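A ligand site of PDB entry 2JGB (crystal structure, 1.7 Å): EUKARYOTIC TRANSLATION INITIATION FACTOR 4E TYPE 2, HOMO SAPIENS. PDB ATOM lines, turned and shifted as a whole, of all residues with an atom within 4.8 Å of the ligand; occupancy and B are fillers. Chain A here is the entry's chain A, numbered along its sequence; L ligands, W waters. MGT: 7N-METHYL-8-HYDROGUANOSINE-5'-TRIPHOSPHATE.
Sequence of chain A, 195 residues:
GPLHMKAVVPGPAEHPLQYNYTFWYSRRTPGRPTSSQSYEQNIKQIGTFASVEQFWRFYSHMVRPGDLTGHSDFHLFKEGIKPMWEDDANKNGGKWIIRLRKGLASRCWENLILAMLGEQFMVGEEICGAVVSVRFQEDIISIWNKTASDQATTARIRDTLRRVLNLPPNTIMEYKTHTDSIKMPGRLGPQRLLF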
ATOM      1  N   ARG A  28      10.216  27.909 -27.853  1.00  0.00           N
ATOM      2  CA  ARG A  28      10.499  27.572 -26.452  1.00  0.00           C
ATOM      3  C   ARG A  28      11.847  26.881 -26.361  1.00  0.00           C
ATOM      4  O   ARG A  28      12.608  26.912 -27.313  1.00  0.00           O
ATOM      5  CB  ARG A  28       9.364  26.739 -25.828  1.00  0.00           C
ATOM      6  CG  ARG A  28       9.004  25.496 -26.553  1.00  0.00           C
ATOM      7  CD  ARG A  28       7.587  25.051 -26.142  1.00  0.00           C
ATOM      8  NE  ARG A  28       6.725  24.863 -27.311  1.00  0.00           N
ATOM      9  CZ  ARG A  28       5.545  25.428 -27.520  1.00  0.00           C
ATOM     10  NH1 ARG A  28       4.970  26.234 -26.619  1.00  0.00           N
ATOM     11  NH2 ARG A  28       4.888  25.151 -28.643  1.00  0.00           N
ATOM     12  N   PRO A  30      13.716  23.004 -25.045  1.00  0.00           N
ATOM     13  CA  PRO A  30      13.278  21.627 -24.751  1.00  0.00           C
ATOM     14  C   PRO A  30      13.230  21.365 -23.254  1.00  0.00           C
ATOM     15  O   PRO A  30      14.015  21.942 -22.510  1.00  0.00           O
ATOM     16  CB  PRO A  30      14.403  20.779 -25.376  1.00  0.00           C
ATOM     17  CG  PRO A  30      15.606  21.677 -25.364  1.00  0.00           C
ATOM     18  CD  PRO A  30      15.054  23.047 -25.665  1.00  0.00           C
ATOM     19  N   ARG A  32      10.791  21.758 -20.823  1.00  0.00           N
ATOM     20  CA  ARG A  32      10.070  22.592 -19.868  1.00  0.00           C
ATOM     21  C   ARG A  32       8.941  21.811 -19.218  1.00  0.00           C
ATOM     22  O   ARG A  32       8.219  21.068 -19.908  1.00  0.00           O
ATOM     23  CB  ARG A  32       9.473  23.835 -20.534  1.00  0.00           C
ATOM     24  CG  ARG A  32      10.488  24.856 -20.975  1.00  0.00           C
ATOM     25  CD  ARG A  32       9.808  26.130 -21.453  1.00  0.00           C
ATOM     26  NE  ARG A  32      10.798  27.039 -22.019  1.00  0.00           N
ATOM     27  CZ  ARG A  32      10.528  28.173 -22.657  1.00  0.00           C
ATOM     28  NH1 ARG A  32       9.275  28.574 -22.823  1.00  0.00           N
ATOM     29  NH2 ARG A  32      11.533  28.913 -23.119  1.00  0.00           N
ATOM     30  N   THR A  34       5.557  21.367 -18.446  1.00  0.00           N
ATOM     31  CA  THR A  34       4.550  21.995 -19.290  1.00  0.00           C
ATOM     32  C   THR A  34       3.135  21.545 -18.953  1.00  0.00           C
ATOM     33  O   THR A  34       2.772  20.386 -19.187  1.00  0.00           O
ATOM     34  CB  THR A  34       4.838  21.724 -20.797  1.00  0.00           C
ATOM     35  OG1 THR A  34       6.217  22.009 -21.093  1.00  0.00           O
ATOM     36  CG2 THR A  34       3.939  22.579 -21.684  1.00  0.00           C
ATOM     37  N   SER A  35       2.354  22.469 -18.406  1.00  0.00           N
ATOM     38  CA  SER A  35       0.920  22.257 -18.218  1.00  0.00           C
ATOM     39  C   SER A  35       0.170  22.760 -19.448  1.00  0.00           C
ATOM     40  O   SER A  35       0.781  23.304 -20.374  1.00  0.00           O
ATOM     41  CB  SER A  35       0.451  22.990 -16.952  1.00  0.00           C
ATOM     42  OG  SER A  35       0.585  24.391 -17.090  1.00  0.00           O
ATOM     43  N   SER A  36      -1.160  22.578 -19.446  1.00  0.00           N
ATOM     44  CA  SER A  36      -2.026  23.113 -20.499  1.00  0.00           C
ATOM     45  C   SER A  36      -1.899  24.623 -20.598  1.00  0.00           C
ATOM     46  O   SER A  36      -1.703  25.176 -21.685  1.00  0.00           O
ATOM     47  CB  SER A  36      -3.485  22.762 -20.212  1.00  0.00           C
ATOM     48  OG  SER A  36      -3.658  21.362 -20.155  1.00  0.00           O
ATOM     49  N   TYR A  39       1.565  25.818 -21.852  1.00  0.00           N
ATOM     50  CA  TYR A  39       1.740  25.556 -23.279  1.00  0.00           C
ATOM     51  C   TYR A  39       0.987  26.613 -24.091  1.00  0.00           C
ATOM     52  O   TYR A  39       1.548  27.196 -25.026  1.00  0.00           O
ATOM     53  CB  TYR A  39       1.321  24.122 -23.694  1.00  0.00           C
ATOM     54  CG  TYR A  39       1.691  23.820 -25.129  1.00  0.00           C
ATOM     55  CD1 TYR A  39       2.957  23.301 -25.450  1.00  0.00           C
ATOM     56  CD2 TYR A  39       0.802  24.089 -26.177  1.00  0.00           C
ATOM     57  CE1 TYR A  39       3.316  23.038 -26.775  1.00  0.00           C
ATOM     58  CE2 TYR A  39       1.150  23.835 -27.505  1.00  0.00           C
ATOM     59  CZ  TYR A  39       2.399  23.320 -27.795  1.00  0.00           C
ATOM     60  OH  TYR A  39       2.726  23.066 -29.115  1.00  0.00           O
ATOM     61  N   HIS A  71      14.296  26.535 -31.054  1.00  0.00           N
ATOM     62  CA  HIS A  71      13.337  25.415 -30.927  1.00  0.00           C
ATOM     63  C   HIS A  71      11.963  26.042 -31.165  1.00  0.00           C
ATOM     64  O   HIS A  71      11.300  26.543 -30.224  1.00  0.00           O
ATOM     65  CB  HIS A  71      13.469  24.886 -29.497  1.00  0.00           C
ATOM     66  CG  HIS A  71      12.535  23.764 -29.128  1.00  0.00           C
ATOM     67  ND1 HIS A  71      13.005  22.499 -28.801  1.00  0.00           N
ATOM     68  CD2 HIS A  71      11.183  23.718 -28.972  1.00  0.00           C
ATOM     69  CE1 HIS A  71      11.977  21.734 -28.452  1.00  0.00           C
ATOM     70  NE2 HIS A  71      10.868  22.452 -28.540  1.00  0.00           N
ATOM     71  N   ASP A  73       8.312  26.472 -33.953  1.00  0.00           N
ATOM     72  CA  ASP A  73       7.342  25.705 -34.763  1.00  0.00           C
ATOM     73  C   ASP A  73       6.341  26.658 -35.426  1.00  0.00           C
ATOM     74  O   ASP A  73       5.985  27.718 -34.843  1.00  0.00           O
ATOM     75  CB  ASP A  73       6.499  24.772 -33.889  1.00  0.00           C
ATOM     76  CG  ASP A  73       7.319  23.825 -32.967  1.00  0.00           C
ATOM     77  OD1 ASP A  73       7.072  22.624 -33.049  1.00  0.00           O
ATOM     78  OD2 ASP A  73       8.111  24.279 -32.128  1.00  0.00           O
ATOM     79  N   PRO A  83      -3.901  24.276 -31.608  1.00  0.00           N
ATOM     80  CA  PRO A  83      -2.907  23.186 -31.831  1.00  0.00           C
ATOM     81  C   PRO A  83      -2.433  22.536 -30.539  1.00  0.00           C
ATOM     82  O   PRO A  83      -1.218  22.479 -30.275  1.00  0.00           O
ATOM     83  CB  PRO A  83      -1.757  23.878 -32.574  1.00  0.00           C
ATOM     84  CG  PRO A  83      -1.838  25.310 -32.202  1.00  0.00           C
ATOM     85  CD  PRO A  83      -3.313  25.614 -31.843  1.00  0.00           C
ATOM     86  N   MET A  84      -3.401  22.080 -29.751  1.00  0.00           N
ATOM     87  CA  MET A  84      -3.139  21.436 -28.467  1.00  0.00           C
ATOM     88  C   MET A  84      -3.960  20.164 -28.305  1.00  0.00           C
ATOM     89  O   MET A  84      -5.124  20.105 -28.735  1.00  0.00           O
ATOM     90  CB  MET A  84      -3.455  22.398 -27.318  1.00  0.00           C
ATOM     91  CG  MET A  84      -2.672  23.702 -27.365  1.00  0.00           C
ATOM     92  SD  MET A  84      -3.228  24.799 -26.033  1.00  0.00           S
ATOM     93  CE  MET A  84      -2.702  23.848 -24.592  1.00  0.00           C
ATOM     94  N   TRP A  85      -3.357  19.163 -27.649  1.00  0.00           N
ATOM     95  CA  TRP A  85      -4.036  17.883 -27.302  1.00  0.00           C
ATOM     96  C   TRP A  85      -5.362  18.104 -26.563  1.00  0.00           C
ATOM     97  O   TRP A  85      -6.331  17.357 -26.763  1.00  0.00           O
ATOM     98  CB  TRP A  85      -3.139  17.024 -26.394  1.00  0.00           C
ATOM     99  CG  TRP A  85      -1.787  16.748 -26.886  1.00  0.00           C
ATOM    100  CD1 TRP A  85      -1.384  16.559 -28.184  1.00  0.00           C
ATOM    101  CD2 TRP A  85      -0.622  16.578 -26.081  1.00  0.00           C
ATOM    102  NE1 TRP A  85      -0.041  16.309 -28.228  1.00  0.00           N
ATOM    103  CE2 TRP A  85       0.455  16.301 -26.956  1.00  0.00           C
ATOM    104  CE3 TRP A  85      -0.377  16.644 -24.693  1.00  0.00           C
ATOM    105  CZ2 TRP A  85       1.768  16.086 -26.491  1.00  0.00           C
ATOM    106  CZ3 TRP A  85       0.938  16.417 -24.235  1.00  0.00           C
ATOM    107  CH2 TRP A  85       1.979  16.148 -25.130  1.00  0.00           C
ATOM    108  N   GLU A  86      -5.409  19.124 -25.714  1.00  0.00           N
ATOM    109  CA  GLU A  86      -6.569  19.417 -24.860  1.00  0.00           C
ATOM    110  C   GLU A  86      -7.795  19.915 -25.629  1.00  0.00           C
ATOM    111  O   GLU A  86      -8.905  19.884 -25.093  1.00  0.00           O
ATOM    112  CB  GLU A  86      -6.196  20.462 -23.809  1.00  0.00           C
ATOM    113  CG  GLU A  86      -5.242  19.928 -22.762  1.00  0.00           C
ATOM    114  CD  GLU A  86      -3.762  20.053 -23.111  1.00  0.00           C
ATOM    115  OE1 GLU A  86      -3.376  20.392 -24.252  1.00  0.00           O
ATOM    116  OE2 GLU A  86      -2.958  19.757 -22.191  1.00  0.00           O
ATOM    117  N   ARG A 135      14.369  21.893 -35.105  1.00  0.00           N
ATOM    118  CA  ARG A 135      15.087  21.434 -33.900  1.00  0.00           C
ATOM    119  C   ARG A 135      16.597  21.482 -34.157  1.00  0.00           C
ATOM    120  O   ARG A 135      17.008  21.931 -35.211  1.00  0.00           O
ATOM    121  CB  ARG A 135      14.615  20.046 -33.445  1.00  0.00           C
ATOM    122  CG  ARG A 135      13.139  20.004 -33.040  1.00  0.00           C
ATOM    123  CD  ARG A 135      12.837  20.738 -31.759  1.00  0.00           C
ATOM    124  NE  ARG A 135      11.411  20.681 -31.344  1.00  0.00           N
ATOM    125  CZ  ARG A 135      10.471  21.556 -31.726  1.00  0.00           C
ATOM    126  NH1 ARG A 135      10.768  22.538 -32.574  1.00  0.00           N
ATOM    127  NH2 ARG A 135       9.213  21.429 -31.277  1.00  0.00           N
ATOM    128  N   TRP A 144      -2.083  16.363 -37.923  1.00  0.00           N
ATOM    129  CA  TRP A 144      -2.974  15.917 -36.845  1.00  0.00           C
ATOM    130  C   TRP A 144      -4.334  15.573 -37.378  1.00  0.00           C
ATOM    131  O   TRP A 144      -4.889  16.371 -38.153  1.00  0.00           O
ATOM    132  CB  TRP A 144      -3.159  17.041 -35.831  1.00  0.00           C
ATOM    133  CG  TRP A 144      -1.924  17.389 -35.048  1.00  0.00           C
ATOM    134  CD1 TRP A 144      -0.620  17.344 -35.466  1.00  0.00           C
ATOM    135  CD2 TRP A 144      -1.901  17.876 -33.707  1.00  0.00           C
ATOM    136  NE1 TRP A 144       0.227  17.753 -34.443  1.00  0.00           N
ATOM    137  CE2 TRP A 144      -0.537  18.078 -33.350  1.00  0.00           C
ATOM    138  CE3 TRP A 144      -2.907  18.142 -32.755  1.00  0.00           C
ATOM    139  CZ2 TRP A 144      -0.169  18.563 -32.082  1.00  0.00           C
ATOM    140  CZ3 TRP A 144      -2.524  18.618 -31.497  1.00  0.00           C
ATOM    141  CH2 TRP A 144      -1.176  18.819 -31.183  1.00  0.00           C
ATOM    142  N   MET A 184       3.768   9.471 -22.141  1.00  0.00           N
ATOM    143  CA  MET A 184       5.136   9.147 -22.510  1.00  0.00           C
ATOM    144  C   MET A 184       6.122   9.964 -21.654  1.00  0.00           C
ATOM    145  O   MET A 184       5.916  11.167 -21.486  1.00  0.00           O
ATOM    146  CB  MET A 184       5.355   9.479 -23.980  1.00  0.00           C
ATOM    147  CG  MET A 184       6.731   9.188 -24.524  1.00  0.00           C
ATOM    148  SD  MET A 184       7.036  10.251 -25.952  1.00  0.00           S
ATOM    149  CE  MET A 184       7.812  11.687 -25.193  1.00  0.00           C
ATOM    150  N   ARG A 192      18.439  14.517 -22.565  1.00  0.00           N
ATOM    151  CA  ARG A 192      18.559  15.167 -23.871  1.00  0.00           C
ATOM    152  C   ARG A 192      18.736  16.678 -23.712  1.00  0.00           C
ATOM    153  O   ARG A 192      17.800  17.379 -23.319  1.00  0.00           O
ATOM    154  CB  ARG A 192      17.313  14.897 -24.714  1.00  0.00           C
ATOM    155  CG  ARG A 192      17.436  15.329 -26.155  1.00  0.00           C
ATOM    156  CD  ARG A 192      16.078  15.346 -26.787  1.00  0.00           C
ATOM    157  NE  ARG A 192      16.085  14.713 -28.100  1.00  0.00           N
ATOM    158  CZ  ARG A 192      15.005  14.239 -28.720  1.00  0.00           C
ATOM    159  NH1 ARG A 192      13.811  14.331 -28.134  1.00  0.00           N
ATOM    160  NH2 ARG A 192      15.115  13.673 -29.912  1.00  0.00           N
ATOM    161  N   PHE A 195      18.027  20.232 -28.375  1.00  0.00           N
ATOM    162  CA  PHE A 195      16.960  19.817 -29.266  1.00  0.00           C
ATOM    163  C   PHE A 195      16.119  21.024 -29.592  1.00  0.00           C
ATOM    164  O   PHE A 195      16.051  21.469 -30.733  1.00  0.00           O
ATOM    165  CB  PHE A 195      16.093  18.738 -28.609  1.00  0.00           C
ATOM    166  CG  PHE A 195      15.086  18.109 -29.532  1.00  0.00           C
ATOM    167  CD1 PHE A 195      15.494  17.514 -30.724  1.00  0.00           C
ATOM    168  CD2 PHE A 195      13.730  18.074 -29.188  1.00  0.00           C
ATOM    169  CE1 PHE A 195      14.569  16.907 -31.579  1.00  0.00           C
ATOM    170  CE2 PHE A 195      12.795  17.476 -30.047  1.00  0.00           C
ATOM    171  CZ  PHE A 195      13.216  16.884 -31.241  1.00  0.00           C
ATOM    172  OXT PHE A 195      15.492  21.550 -28.698  1.00  0.00           O
HETATM  173  PG  MGT L   1       8.549  15.946 -27.799  1.00  0.00           P
HETATM  174  O1G MGT L   1       8.353  16.062 -26.302  1.00  0.00           O
HETATM  175  O2G MGT L   1       9.301  14.714 -28.233  1.00  0.00           O
HETATM  176  O3G MGT L   1       7.317  16.251 -28.637  1.00  0.00           O
HETATM  177  O3B MGT L   1       9.646  17.090 -28.176  1.00  0.00           O
HETATM  178  PB  MGT L   1       9.627  18.706 -28.225  1.00  0.00           P
HETATM  179  O1B MGT L   1      10.662  19.203 -27.230  1.00  0.00           O
HETATM  180  O2B MGT L   1       9.763  19.118 -29.670  1.00  0.00           O
HETATM  181  O3A MGT L   1       8.195  19.169 -27.649  1.00  0.00           O
HETATM  182  PA  MGT L   1       7.444  20.555 -28.027  1.00  0.00           P
HETATM  183  O1A MGT L   1       8.345  21.767 -28.058  1.00  0.00           O
HETATM  184  O2A MGT L   1       6.604  20.233 -29.231  1.00  0.00           O
HETATM  185  O5' MGT L   1       6.488  20.735 -26.745  1.00  0.00           O
HETATM  186  C5' MGT L   1       7.071  21.147 -25.508  1.00  0.00           C
HETATM  187  C4' MGT L   1       6.530  20.325 -24.343  1.00  0.00           C
HETATM  188  O4' MGT L   1       5.119  20.579 -24.226  1.00  0.00           O
HETATM  189  C3' MGT L   1       6.732  18.825 -24.532  1.00  0.00           C
HETATM  190  O3' MGT L   1       7.025  18.181 -23.282  1.00  0.00           O
HETATM  191  C2' MGT L   1       5.381  18.340 -24.956  1.00  0.00           C
HETATM  192  O2' MGT L   1       5.087  17.029 -24.473  1.00  0.00           O
HETATM  193  C1' MGT L   1       4.419  19.342 -24.350  1.00  0.00           C
HETATM  194  N9  MGT L   1       3.269  19.492 -25.255  1.00  0.00           N
HETATM  195  C8  MGT L   1       3.264  19.435 -26.625  1.00  0.00           C
HETATM  196  N7  MGT L   1       2.013  19.625 -27.115  1.00  0.00           N
HETATM  197  CM7 MGT L   1       1.632  19.612 -28.557  1.00  0.00           C
HETATM  198  C5  MGT L   1       1.234  19.800 -26.040  1.00  0.00           C
HETATM  199  C6  MGT L   1      -0.205  20.048 -25.881  1.00  0.00           C
HETATM  200  O6  MGT L   1      -0.942  20.100 -26.876  1.00  0.00           O
HETATM  201  N1  MGT L   1      -0.673  20.180 -24.615  1.00  0.00           N
HETATM  202  C2  MGT L   1       0.142  20.096 -23.533  1.00  0.00           C
HETATM  203  N2  MGT L   1      -0.364  20.246 -22.280  1.00  0.00           N
HETATM  204  N3  MGT L   1       1.473  19.881 -23.625  1.00  0.00           N
HETATM  205  C4  MGT L   1       2.043  19.722 -24.833  1.00  0.00           C
HETATM  206  O   HOH W   1       8.827  19.257 -21.632  1.00  0.00           O
HETATM  207  O   HOH W   2      10.095  14.998 -31.462  1.00  0.00           O
HETATM  208  O   HOH W   3       9.556  17.589 -31.815  1.00  0.00           O
HETATM  209  O   HOH W   4       5.545  17.924 -29.373  1.00  0.00           O
HETATM  210  O   HOH W   5      10.246  19.720 -24.655  1.00  0.00           O
HETATM  211  O   HOH W   6       4.814  15.756 -27.517  1.00  0.00           O
HETATM  212  O   HOH W   7       3.254  17.691 -30.706  1.00  0.00           O
HETATM  213  O   HOH W   8       5.258  21.482 -31.094  1.00  0.00           O
HETATM  214  O   HOH W   9      12.762  17.450 -25.802  1.00  0.00           O
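Thr 34 touches the ligand.
Ser 35 touches the ligand (O to N2, 3.8 Å).
Ser 36 touches the ligand (N to N2, 3.8 Å).
Tyr 39 touches the ligand.
CA of Met 84 touches O6 of the ligand (3.0 Å).
CH2 of Trp 144 touches CM7 of the ligand, 3.9 Å away.
CE2 of Phe 195 touches O2B of the ligand (3.5 Å).
Hydrophobic or aromatic side chains within 4 Å of the ligand: Tyr 39, His 71, Met 84, Trp 85, Trp 144 and Phe 195.
12 residues have an atom within 4 Å of the ligand: Arg 28, Thr 34, Ser 35, Ser 36, Tyr 39, His 71, Met 84, Trp 85, Glu 86, Arg 135, Trp 144 and Phe 195.
The nearest printed residue that does not touch the ligand is Pro 83 (4.2 Å).
Water W8 lies within hydrogen-bond range of an oxygen (O2A) of the ligand (2.6 Å) and the side-chain carboxylate (OD1) of Asp 73 (2.9 Å).
Water W1 lies within hydrogen-bond range of the backbone carbonyl oxygen of Arg 32 (2.6 Å) and an oxygen (O3') of the ligand (2.7 Å).
The side-chain hydroxyl (OG) of Ser 36 is in hydrogen-bond range of the side-chain carboxylate (OE2) of Glu 86, 2.7 Å away.
NH2 of Arg 135 sits close to NE2 of His 71, 3.4 Å away.
OXT of Phe 195 sits at hydrogen-bond distance from ND1 of His 71.
The backbone carbonyl oxygen (O) of His 71 sits at hydrogen-bond distance from the backbone NH (N) of Arg 28, at 2.9 Å.
The guanidinium group of Arg 135 lies within salt-bridge range of the side-chain carboxylate of Asp 73, 3.0 Å away.
The backbone carbonyl oxygen (O) of Arg 32 lies within hydrogen-bond range of the side-chain hydroxyl (OG1) of Thr 34, at 2.5 Å.
The guanidinium group (NH2) of Arg 28 is in hydrogen-bond range of the side-chain hydroxyl (OH) of Tyr 39, 3.0 Å away.
A nitrogen (N2) of the ligand sits at hydrogen-bond distance from the side-chain carboxylate (OE2) of Glu 86 (2.6 Å).
An oxygen (O1A) of the ligand lies within hydrogen-bond range of a ring nitrogen (NE2) of His 71.
An oxygen (O6) of the ligand lies within hydrogen-bond range of the backbone NH of Trp 85.
An oxygen (O2B) of the ligand is in salt-bridge range of the guanidinium group (NE) of Arg 135 (2.8 Å).
The guanidinium group of Arg 28 is in salt-bridge range of an oxygen (O1A) of the ligand (3.6 Å).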
